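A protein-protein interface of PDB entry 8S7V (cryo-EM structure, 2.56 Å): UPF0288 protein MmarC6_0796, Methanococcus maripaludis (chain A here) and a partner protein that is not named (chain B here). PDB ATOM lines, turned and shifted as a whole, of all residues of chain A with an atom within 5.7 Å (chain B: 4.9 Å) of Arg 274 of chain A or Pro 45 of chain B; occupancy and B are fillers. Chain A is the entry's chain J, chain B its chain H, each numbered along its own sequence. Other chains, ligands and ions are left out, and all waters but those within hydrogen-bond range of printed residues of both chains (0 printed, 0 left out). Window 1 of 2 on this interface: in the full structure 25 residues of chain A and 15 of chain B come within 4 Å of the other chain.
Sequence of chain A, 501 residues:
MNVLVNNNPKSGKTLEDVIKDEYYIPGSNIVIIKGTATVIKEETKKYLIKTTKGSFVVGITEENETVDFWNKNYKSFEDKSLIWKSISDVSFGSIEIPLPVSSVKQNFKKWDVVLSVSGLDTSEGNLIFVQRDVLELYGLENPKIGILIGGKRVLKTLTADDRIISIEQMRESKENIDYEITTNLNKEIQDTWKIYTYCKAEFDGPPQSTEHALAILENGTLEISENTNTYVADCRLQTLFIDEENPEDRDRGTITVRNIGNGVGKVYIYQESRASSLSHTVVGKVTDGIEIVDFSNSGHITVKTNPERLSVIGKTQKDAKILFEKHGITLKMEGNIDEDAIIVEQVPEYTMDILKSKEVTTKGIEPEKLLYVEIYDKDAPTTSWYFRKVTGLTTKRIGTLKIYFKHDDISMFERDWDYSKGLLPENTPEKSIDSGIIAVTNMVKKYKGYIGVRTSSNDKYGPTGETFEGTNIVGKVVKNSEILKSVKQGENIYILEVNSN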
ATOM      1  N   ASN A 229     -35.202   8.657   0.262  1.00  0.00           N
ATOM      2  CA  ASN A 229     -34.559   8.736  -1.041  1.00  0.00           C
ATOM      3  C   ASN A 229     -33.280   7.914  -1.119  1.00  0.00           C
ATOM      4  O   ASN A 229     -32.692   7.820  -2.200  1.00  0.00           O
ATOM      5  CB  ASN A 229     -34.258  10.194  -1.391  1.00  0.00           C
ATOM      6  CG  ASN A 229     -35.500  10.967  -1.780  1.00  0.00           C
ATOM      7  OD1 ASN A 229     -36.464  10.398  -2.291  1.00  0.00           O
ATOM      8  ND2 ASN A 229     -35.485  12.272  -1.537  1.00  0.00           N
ATOM      9  N   THR A 230     -32.836   7.323  -0.009  1.00  0.00           N
ATOM     10  CA  THR A 230     -31.588   6.573   0.022  1.00  0.00           C
ATOM     11  C   THR A 230     -31.741   5.113   0.417  1.00  0.00           C
ATOM     12  O   THR A 230     -30.864   4.312   0.089  1.00  0.00           O
ATOM     13  CB  THR A 230     -30.589   7.231   0.983  1.00  0.00           C
ATOM     14  OG1 THR A 230     -31.056   7.095   2.329  1.00  0.00           O
ATOM     15  CG2 THR A 230     -30.413   8.702   0.653  1.00  0.00           C
ATOM     16  N   ASP A 249     -18.596   0.261   3.558  1.00  0.00           N
ATOM     17  CA  ASP A 249     -19.381   1.207   2.776  1.00  0.00           C
ATOM     18  C   ASP A 249     -20.773   0.663   2.481  1.00  0.00           C
ATOM     19  O   ASP A 249     -20.934  -0.500   2.101  1.00  0.00           O
ATOM     20  CB  ASP A 249     -18.657   1.529   1.470  1.00  0.00           C
ATOM     21  CG  ASP A 249     -17.742   2.727   1.594  1.00  0.00           C
ATOM     22  OD1 ASP A 249     -17.130   2.901   2.669  1.00  0.00           O
ATOM     23  OD2 ASP A 249     -17.633   3.497   0.618  1.00  0.00           O
ATOM     24  N   ARG A 250     -21.783   1.517   2.661  1.00  0.00           N
ATOM     25  CA  ARG A 250     -23.166   1.184   2.327  1.00  0.00           C
ATOM     26  C   ARG A 250     -23.410   1.595   0.878  1.00  0.00           C
ATOM     27  O   ARG A 250     -24.014   2.626   0.577  1.00  0.00           O
ATOM     28  CB  ARG A 250     -24.129   1.872   3.285  1.00  0.00           C
ATOM     29  CG  ARG A 250     -23.948   1.471   4.736  1.00  0.00           C
ATOM     30  CD  ARG A 250     -24.841   2.288   5.651  1.00  0.00           C
ATOM     31  NE  ARG A 250     -24.335   3.642   5.840  1.00  0.00           N
ATOM     32  CZ  ARG A 250     -24.979   4.596   6.499  1.00  0.00           C
ATOM     33  NH1 ARG A 250     -26.164   4.381   7.044  1.00  0.00           N
ATOM     34  NH2 ARG A 250     -24.417   5.795   6.615  1.00  0.00           N
ATOM     35  N   ASP A 251     -22.924   0.759  -0.035  1.00  0.00           N
ATOM     36  CA  ASP A 251     -22.947   1.075  -1.457  1.00  0.00           C
ATOM     37  C   ASP A 251     -24.350   0.871  -2.025  1.00  0.00           C
ATOM     38  O   ASP A 251     -25.324   0.651  -1.302  1.00  0.00           O
ATOM     39  CB  ASP A 251     -21.917   0.232  -2.202  1.00  0.00           C
ATOM     40  CG  ASP A 251     -20.537   0.324  -1.592  1.00  0.00           C
ATOM     41  OD1 ASP A 251     -20.024   1.452  -1.452  1.00  0.00           O
ATOM     42  OD2 ASP A 251     -19.963  -0.733  -1.254  1.00  0.00           O
ATOM     43  N   TYR A 270     -30.047  -0.186   0.649  1.00  0.00           N
ATOM     44  CA  TYR A 270     -29.652   1.168   0.281  1.00  0.00           C
ATOM     45  C   TYR A 270     -29.720   1.358  -1.228  1.00  0.00           C
ATOM     46  O   TYR A 270     -29.162   0.562  -1.989  1.00  0.00           O
ATOM     47  CB  TYR A 270     -28.242   1.468   0.787  1.00  0.00           C
ATOM     48  CG  TYR A 270     -28.211   1.995   2.202  1.00  0.00           C
ATOM     49  CD1 TYR A 270     -28.303   1.134   3.286  1.00  0.00           C
ATOM     50  CD2 TYR A 270     -28.105   3.355   2.454  1.00  0.00           C
ATOM     51  CE1 TYR A 270     -28.279   1.613   4.579  1.00  0.00           C
ATOM     52  CE2 TYR A 270     -28.083   3.841   3.743  1.00  0.00           C
ATOM     53  CZ  TYR A 270     -28.171   2.965   4.801  1.00  0.00           C
ATOM     54  OH  TYR A 270     -28.148   3.448   6.089  1.00  0.00           O
ATOM     55  N   GLU A 272     -28.612   4.259  -2.569  1.00  0.00           N
ATOM     56  CA  GLU A 272     -27.606   5.266  -2.875  1.00  0.00           C
ATOM     57  C   GLU A 272     -26.291   4.877  -2.219  1.00  0.00           C
ATOM     58  O   GLU A 272     -26.270   4.208  -1.184  1.00  0.00           O
ATOM     59  CB  GLU A 272     -28.037   6.658  -2.398  1.00  0.00           C
ATOM     60  CG  GLU A 272     -29.287   7.188  -3.074  1.00  0.00           C
ATOM     61  CD  GLU A 272     -28.976   8.138  -4.210  1.00  0.00           C
ATOM     62  OE1 GLU A 272     -27.884   8.743  -4.200  1.00  0.00           O
ATOM     63  OE2 GLU A 272     -29.826   8.281  -5.114  1.00  0.00           O
ATOM     64  N   SER A 273     -25.192   5.309  -2.831  1.00  0.00           N
ATOM     65  CA  SER A 273     -23.854   5.023  -2.316  1.00  0.00           C
ATOM     66  C   SER A 273     -23.564   5.985  -1.172  1.00  0.00           C
ATOM     67  O   SER A 273     -23.358   7.181  -1.386  1.00  0.00           O
ATOM     68  CB  SER A 273     -22.814   5.145  -3.422  1.00  0.00           C
ATOM     69  OG  SER A 273     -23.014   4.164  -4.424  1.00  0.00           O
ATOM     70  N   ARG A 274     -23.551   5.465   0.050  1.00  0.00           N
ATOM     71  CA  ARG A 274     -23.318   6.260   1.245  1.00  0.00           C
ATOM     72  C   ARG A 274     -22.077   5.767   1.977  1.00  0.00           C
ATOM     73  O   ARG A 274     -21.481   4.745   1.631  1.00  0.00           O
ATOM     74  CB  ARG A 274     -24.540   6.218   2.169  1.00  0.00           C
ATOM     75  CG  ARG A 274     -25.809   6.739   1.522  1.00  0.00           C
ATOM     76  CD  ARG A 274     -26.109   8.152   1.982  1.00  0.00           C
ATOM     77  NE  ARG A 274     -27.067   8.828   1.116  1.00  0.00           N
ATOM     78  CZ  ARG A 274     -26.750   9.443  -0.015  1.00  0.00           C
ATOM     79  NH1 ARG A 274     -25.502   9.483  -0.453  1.00  0.00           N
ATOM     80  NH2 ARG A 274     -27.708  10.033  -0.723  1.00  0.00           N
ATOM     81  N   ALA A 275     -21.693   6.519   3.004  1.00  0.00           N
ATOM     82  CA  ALA A 275     -20.498   6.211   3.771  1.00  0.00           C
ATOM     83  C   ALA A 275     -20.769   5.092   4.773  1.00  0.00           C
ATOM     84  O   ALA A 275     -21.914   4.735   5.061  1.00  0.00           O
ATOM     85  CB  ALA A 275     -19.991   7.457   4.492  1.00  0.00           C
ATOM     86  N   SER A 276     -19.687   4.535   5.305  1.00  0.00           N
ATOM     87  CA  SER A 276     -19.791   3.495   6.316  1.00  0.00           C
ATOM     88  C   SER A 276     -20.376   4.055   7.608  1.00  0.00           C
ATOM     89  O   SER A 276     -20.228   5.237   7.924  1.00  0.00           O
ATOM     90  CB  SER A 276     -18.419   2.880   6.589  1.00  0.00           C
ATOM     91  OG  SER A 276     -18.423   2.143   7.797  1.00  0.00           O
ATOM     92  N   MET B   1     -22.972  18.558  -2.826  1.00  0.00           N
ATOM     93  CA  MET B   1     -23.782  17.365  -2.636  1.00  0.00           C
ATOM     94  C   MET B   1     -24.328  17.403  -1.207  1.00  0.00           C
ATOM     95  O   MET B   1     -25.522  17.212  -0.975  1.00  0.00           O
ATOM     96  CB  MET B   1     -22.947  16.102  -2.883  1.00  0.00           C
ATOM     97  CG  MET B   1     -23.546  14.774  -2.407  1.00  0.00           C
ATOM     98  SD  MET B   1     -25.346  14.646  -2.513  1.00  0.00           S
ATOM     99  CE  MET B   1     -25.565  12.873  -2.607  1.00  0.00           C
ATOM    100  N   TYR B   2     -23.443  17.685  -0.256  1.00  0.00           N
ATOM    101  CA  TYR B   2     -23.769  17.670   1.168  1.00  0.00           C
ATOM    102  C   TYR B   2     -23.992  19.113   1.613  1.00  0.00           C
ATOM    103  O   TYR B   2     -23.047  19.829   1.940  1.00  0.00           O
ATOM    104  CB  TYR B   2     -22.642  17.019   1.960  1.00  0.00           C
ATOM    105  CG  TYR B   2     -22.620  15.510   1.909  1.00  0.00           C
ATOM    106  CD1 TYR B   2     -23.682  14.758   2.391  1.00  0.00           C
ATOM    107  CD2 TYR B   2     -21.536  14.836   1.367  1.00  0.00           C
ATOM    108  CE1 TYR B   2     -23.656  13.378   2.341  1.00  0.00           C
ATOM    109  CE2 TYR B   2     -21.506  13.458   1.310  1.00  0.00           C
ATOM    110  CZ  TYR B   2     -22.568  12.734   1.799  1.00  0.00           C
ATOM    111  OH  TYR B   2     -22.542  11.359   1.745  1.00  0.00           O
ATOM    112  N   VAL B  24     -29.831   8.003   6.817  1.00  0.00           N
ATOM    113  CA  VAL B  24     -29.831   8.611   5.487  1.00  0.00           C
ATOM    114  C   VAL B  24     -28.445   9.022   5.028  1.00  0.00           C
ATOM    115  O   VAL B  24     -28.304   9.529   3.907  1.00  0.00           O
ATOM    116  CB  VAL B  24     -30.759   9.840   5.422  1.00  0.00           C
ATOM    117  CG1 VAL B  24     -32.154   9.472   5.893  1.00  0.00           C
ATOM    118  CG2 VAL B  24     -30.192  10.981   6.243  1.00  0.00           C
ATOM    119  N   GLY B  25     -27.418   8.821   5.847  1.00  0.00           N
ATOM    120  CA  GLY B  25     -26.057   9.091   5.440  1.00  0.00           C
ATOM    121  C   GLY B  25     -25.514  10.452   5.806  1.00  0.00           C
ATOM    122  O   GLY B  25     -24.433  10.815   5.329  1.00  0.00           O
ATOM    123  N   GLY B  26     -26.219  11.220   6.630  1.00  0.00           N
ATOM    124  CA  GLY B  26     -25.720  12.516   7.030  1.00  0.00           C
ATOM    125  C   GLY B  26     -24.653  12.422   8.103  1.00  0.00           C
ATOM    126  O   GLY B  26     -24.389  11.366   8.677  1.00  0.00           O
ATOM    127  N   ALA B  43     -24.594  17.937   8.015  1.00  0.00           N
ATOM    128  CA  ALA B  43     -24.353  17.892   6.577  1.00  0.00           C
ATOM    129  C   ALA B  43     -25.031  16.645   6.024  1.00  0.00           C
ATOM    130  O   ALA B  43     -24.606  15.522   6.311  1.00  0.00           O
ATOM    131  CB  ALA B  43     -22.858  17.884   6.272  1.00  0.00           C
ATOM    132  N   ILE B  44     -26.077  16.843   5.233  1.00  0.00           N
ATOM    133  CA  ILE B  44     -26.852  15.739   4.674  1.00  0.00           C
ATOM    134  C   ILE B  44     -26.899  15.917   3.163  1.00  0.00           C
ATOM    135  O   ILE B  44     -26.723  17.034   2.648  1.00  0.00           O
ATOM    136  CB  ILE B  44     -28.272  15.667   5.285  1.00  0.00           C
ATOM    137  CG1 ILE B  44     -29.182  16.725   4.666  1.00  0.00           C
ATOM    138  CG2 ILE B  44     -28.226  15.820   6.792  1.00  0.00           C
ATOM    139  CD1 ILE B  44     -30.622  16.297   4.585  1.00  0.00           C
ATOM    140  N   PRO B  45     -27.118  14.833   2.416  1.00  0.00           N
ATOM    141  CA  PRO B  45     -27.213  14.954   0.956  1.00  0.00           C
ATOM    142  C   PRO B  45     -28.385  15.830   0.541  1.00  0.00           C
ATOM    143  O   PRO B  45     -29.411  15.898   1.221  1.00  0.00           O
ATOM    144  CB  PRO B  45     -27.411  13.507   0.490  1.00  0.00           C
ATOM    145  CG  PRO B  45     -26.905  12.669   1.605  1.00  0.00           C
ATOM    146  CD  PRO B  45     -27.196  13.431   2.857  1.00  0.00           C
ATOM    147  N   GLN B  46     -28.220  16.506  -0.600  1.00  0.00           N
ATOM    148  CA  GLN B  46     -29.244  17.427  -1.077  1.00  0.00           C
ATOM    149  C   GLN B  46     -30.557  16.730  -1.409  1.00  0.00           C
ATOM    150  O   GLN B  46     -31.617  17.357  -1.303  1.00  0.00           O
ATOM    151  CB  GLN B  46     -28.748  18.191  -2.308  1.00  0.00           C
ATOM    152  CG  GLN B  46     -28.167  19.562  -1.997  1.00  0.00           C
ATOM    153  CD  GLN B  46     -26.866  19.828  -2.726  1.00  0.00           C
ATOM    154  OE1 GLN B  46     -26.378  18.983  -3.474  1.00  0.00           O
ATOM    155  NE2 GLN B  46     -26.298  21.008  -2.510  1.00  0.00           N
ATOM    156  N   ASN B  47     -30.521  15.457  -1.795  1.00  0.00           N
ATOM    157  CA  ASN B  47     -31.744  14.750  -2.151  1.00  0.00           C
ATOM    158  C   ASN B  47     -32.594  14.389  -0.941  1.00  0.00           C
ATOM    159  O   ASN B  47     -33.721  13.916  -1.117  1.00  0.00           O
ATOM    160  CB  ASN B  47     -31.414  13.485  -2.949  1.00  0.00           C
ATOM    161  CG  ASN B  47     -30.277  12.692  -2.344  1.00  0.00           C
ATOM    162  OD1 ASN B  47     -29.130  13.139  -2.336  1.00  0.00           O
ATOM    163  ND2 ASN B  47     -30.587  11.507  -1.837  1.00  0.00           N
ATOM    164  N   GLU B  48     -32.088  14.601   0.274  1.00  0.00           N
ATOM    165  CA  GLU B  48     -32.835  14.337   1.496  1.00  0.00           C
ATOM    166  C   GLU B  48     -33.170  15.614   2.258  1.00  0.00           C
ATOM    167  O   GLU B  48     -33.563  15.545   3.426  1.00  0.00           O
ATOM    168  CB  GLU B  48     -32.056  13.378   2.398  1.00  0.00           C
ATOM    169  CG  GLU B  48     -31.871  11.986   1.827  1.00  0.00           C
ATOM    170  CD  GLU B  48     -32.980  11.036   2.233  1.00  0.00           C
ATOM    171  OE1 GLU B  48     -34.149  11.469   2.290  1.00  0.00           O
ATOM    172  OE2 GLU B  48     -32.683   9.857   2.506  1.00  0.00           O
ATOM    173  N   ILE B  49     -33.023  16.778   1.623  1.00  0.00           N
ATOM    174  CA  ILE B  49     -33.252  18.044   2.320  1.00  0.00           C
ATOM    175  C   ILE B  49     -34.715  18.183   2.719  1.00  0.00           C
ATOM    176  O   ILE B  49     -35.034  18.530   3.863  1.00  0.00           O
ATOM    177  CB  ILE B  49     -32.785  19.226   1.453  1.00  0.00           C
ATOM    178  CG1 ILE B  49     -31.267  19.351   1.525  1.00  0.00           C
ATOM    179  CG2 ILE B  49     -33.443  20.515   1.907  1.00  0.00           C
ATOM    180  CD1 ILE B  49     -30.758  19.546   2.930  1.00  0.00           C
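N of Asn 229 of chain A touches OE2 of Glu 48 of chain B, 3.6 Å away. Val 24 of chain B touches Thr 230 of chain A. ND2 of Asn 47 of chain B touches CG2 of Thr 230 of chain A, 3.8 Å away. NH2 of Arg 250 of chain A touches CA of Gly 25 of chain B (3.9 Å). Arg 274 of chain A touches Gly 25 of chain B. Arg 274 of chain A touches Pro 45 of chain B (NH2 to CG, 3.6 Å).
N of Glu 272 of chain A lies within hydrogen-bond range of O of Thr 230 of chain A (3.5 Å). The backbone carbonyl oxygen of Arg 250 of chain A is in hydrogen-bond range of the backbone NH of Arg 274 of chain A, at 2.9 Å. The backbone carbonyl oxygen (O) of Ala 275 of chain A is in hydrogen-bond range of the guanidinium group (NE) of Arg 250 of chain A (2.8 Å). The side-chain carboxylate (OE1) of Glu 272 of chain A lies within salt-bridge range of the guanidinium group (NH2) of Arg 274 of chain A (3.7 Å).
Of the 11 printed residues of chain A, 4 touch a printed residue of chain B. Printed residues of chain A that touch a printed residue of chain B: Asn 229, Thr 230, Arg 250 and Arg 274. Hydrophobic or aromatic side chains of chain B that line the printed part of chain A: Pro 45. Among the printed residues, no Asp or Glu carboxylate lies within 4 Å of a Lys or Arg side-chain nitrogen of the other chain.
O of Val 24 of chain B sits at hydrogen-bond distance from NE of Arg 274 of chain A (3.1 Å). The side-chain hydroxyl (OG1) of Thr 230 of chain A sits close to the side-chain carboxylate (OE2) of Glu 48 of chain B, 3.2 Å away. ND2 of Asn 229 of chain A lies within hydrogen-bond range of O of Asn 47 of chain B (2.4 Å). The guanidinium group (NH2) of Arg 274 of chain A sits close to the side-chain amide nitrogen (ND2) of Asn 47 of chain B.
Of the printed residues of chain B, Arg 274 of chain A touches Val 24 (3.1 Å), Gly 25 (3.6 Å), Pro 45 (3.6 Å) and Asn 47 (3.4 Å). Pro 45 of chain B touches one residue of chain A. Of the printed residues of chain A, Asn 47 of chain B touches Asn 229 (2.4 Å), Thr 230 (3.8 Å) and Arg 274 (3.4 Å). Of the printed residues of chain B, Thr 230 of chain A touches Val 24 (3.7 Å), Asn 47 (3.8 Å) and Glu 48 (3.1 Å). Printed residues of chain A within 4 Å of Gly 25 of chain B: Arg 250 and Arg 274. Ser 276 of chain A touches none of the printed residues of chain B. Tyr 2 of chain B touches none of the printed residues of chain A. The nearest printed residue of chain B that does not touch Arg 274 of chain A is Met 1 of chain B (4.02 Å). The nearest residue of chain A that does not touch Pro 45 of chain B is Thr 230 of chain A (5.4 Å). The nearest printed residue of chain A that does not touch Gly 25 of chain B is Thr 230 of chain A (5.3 Å).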
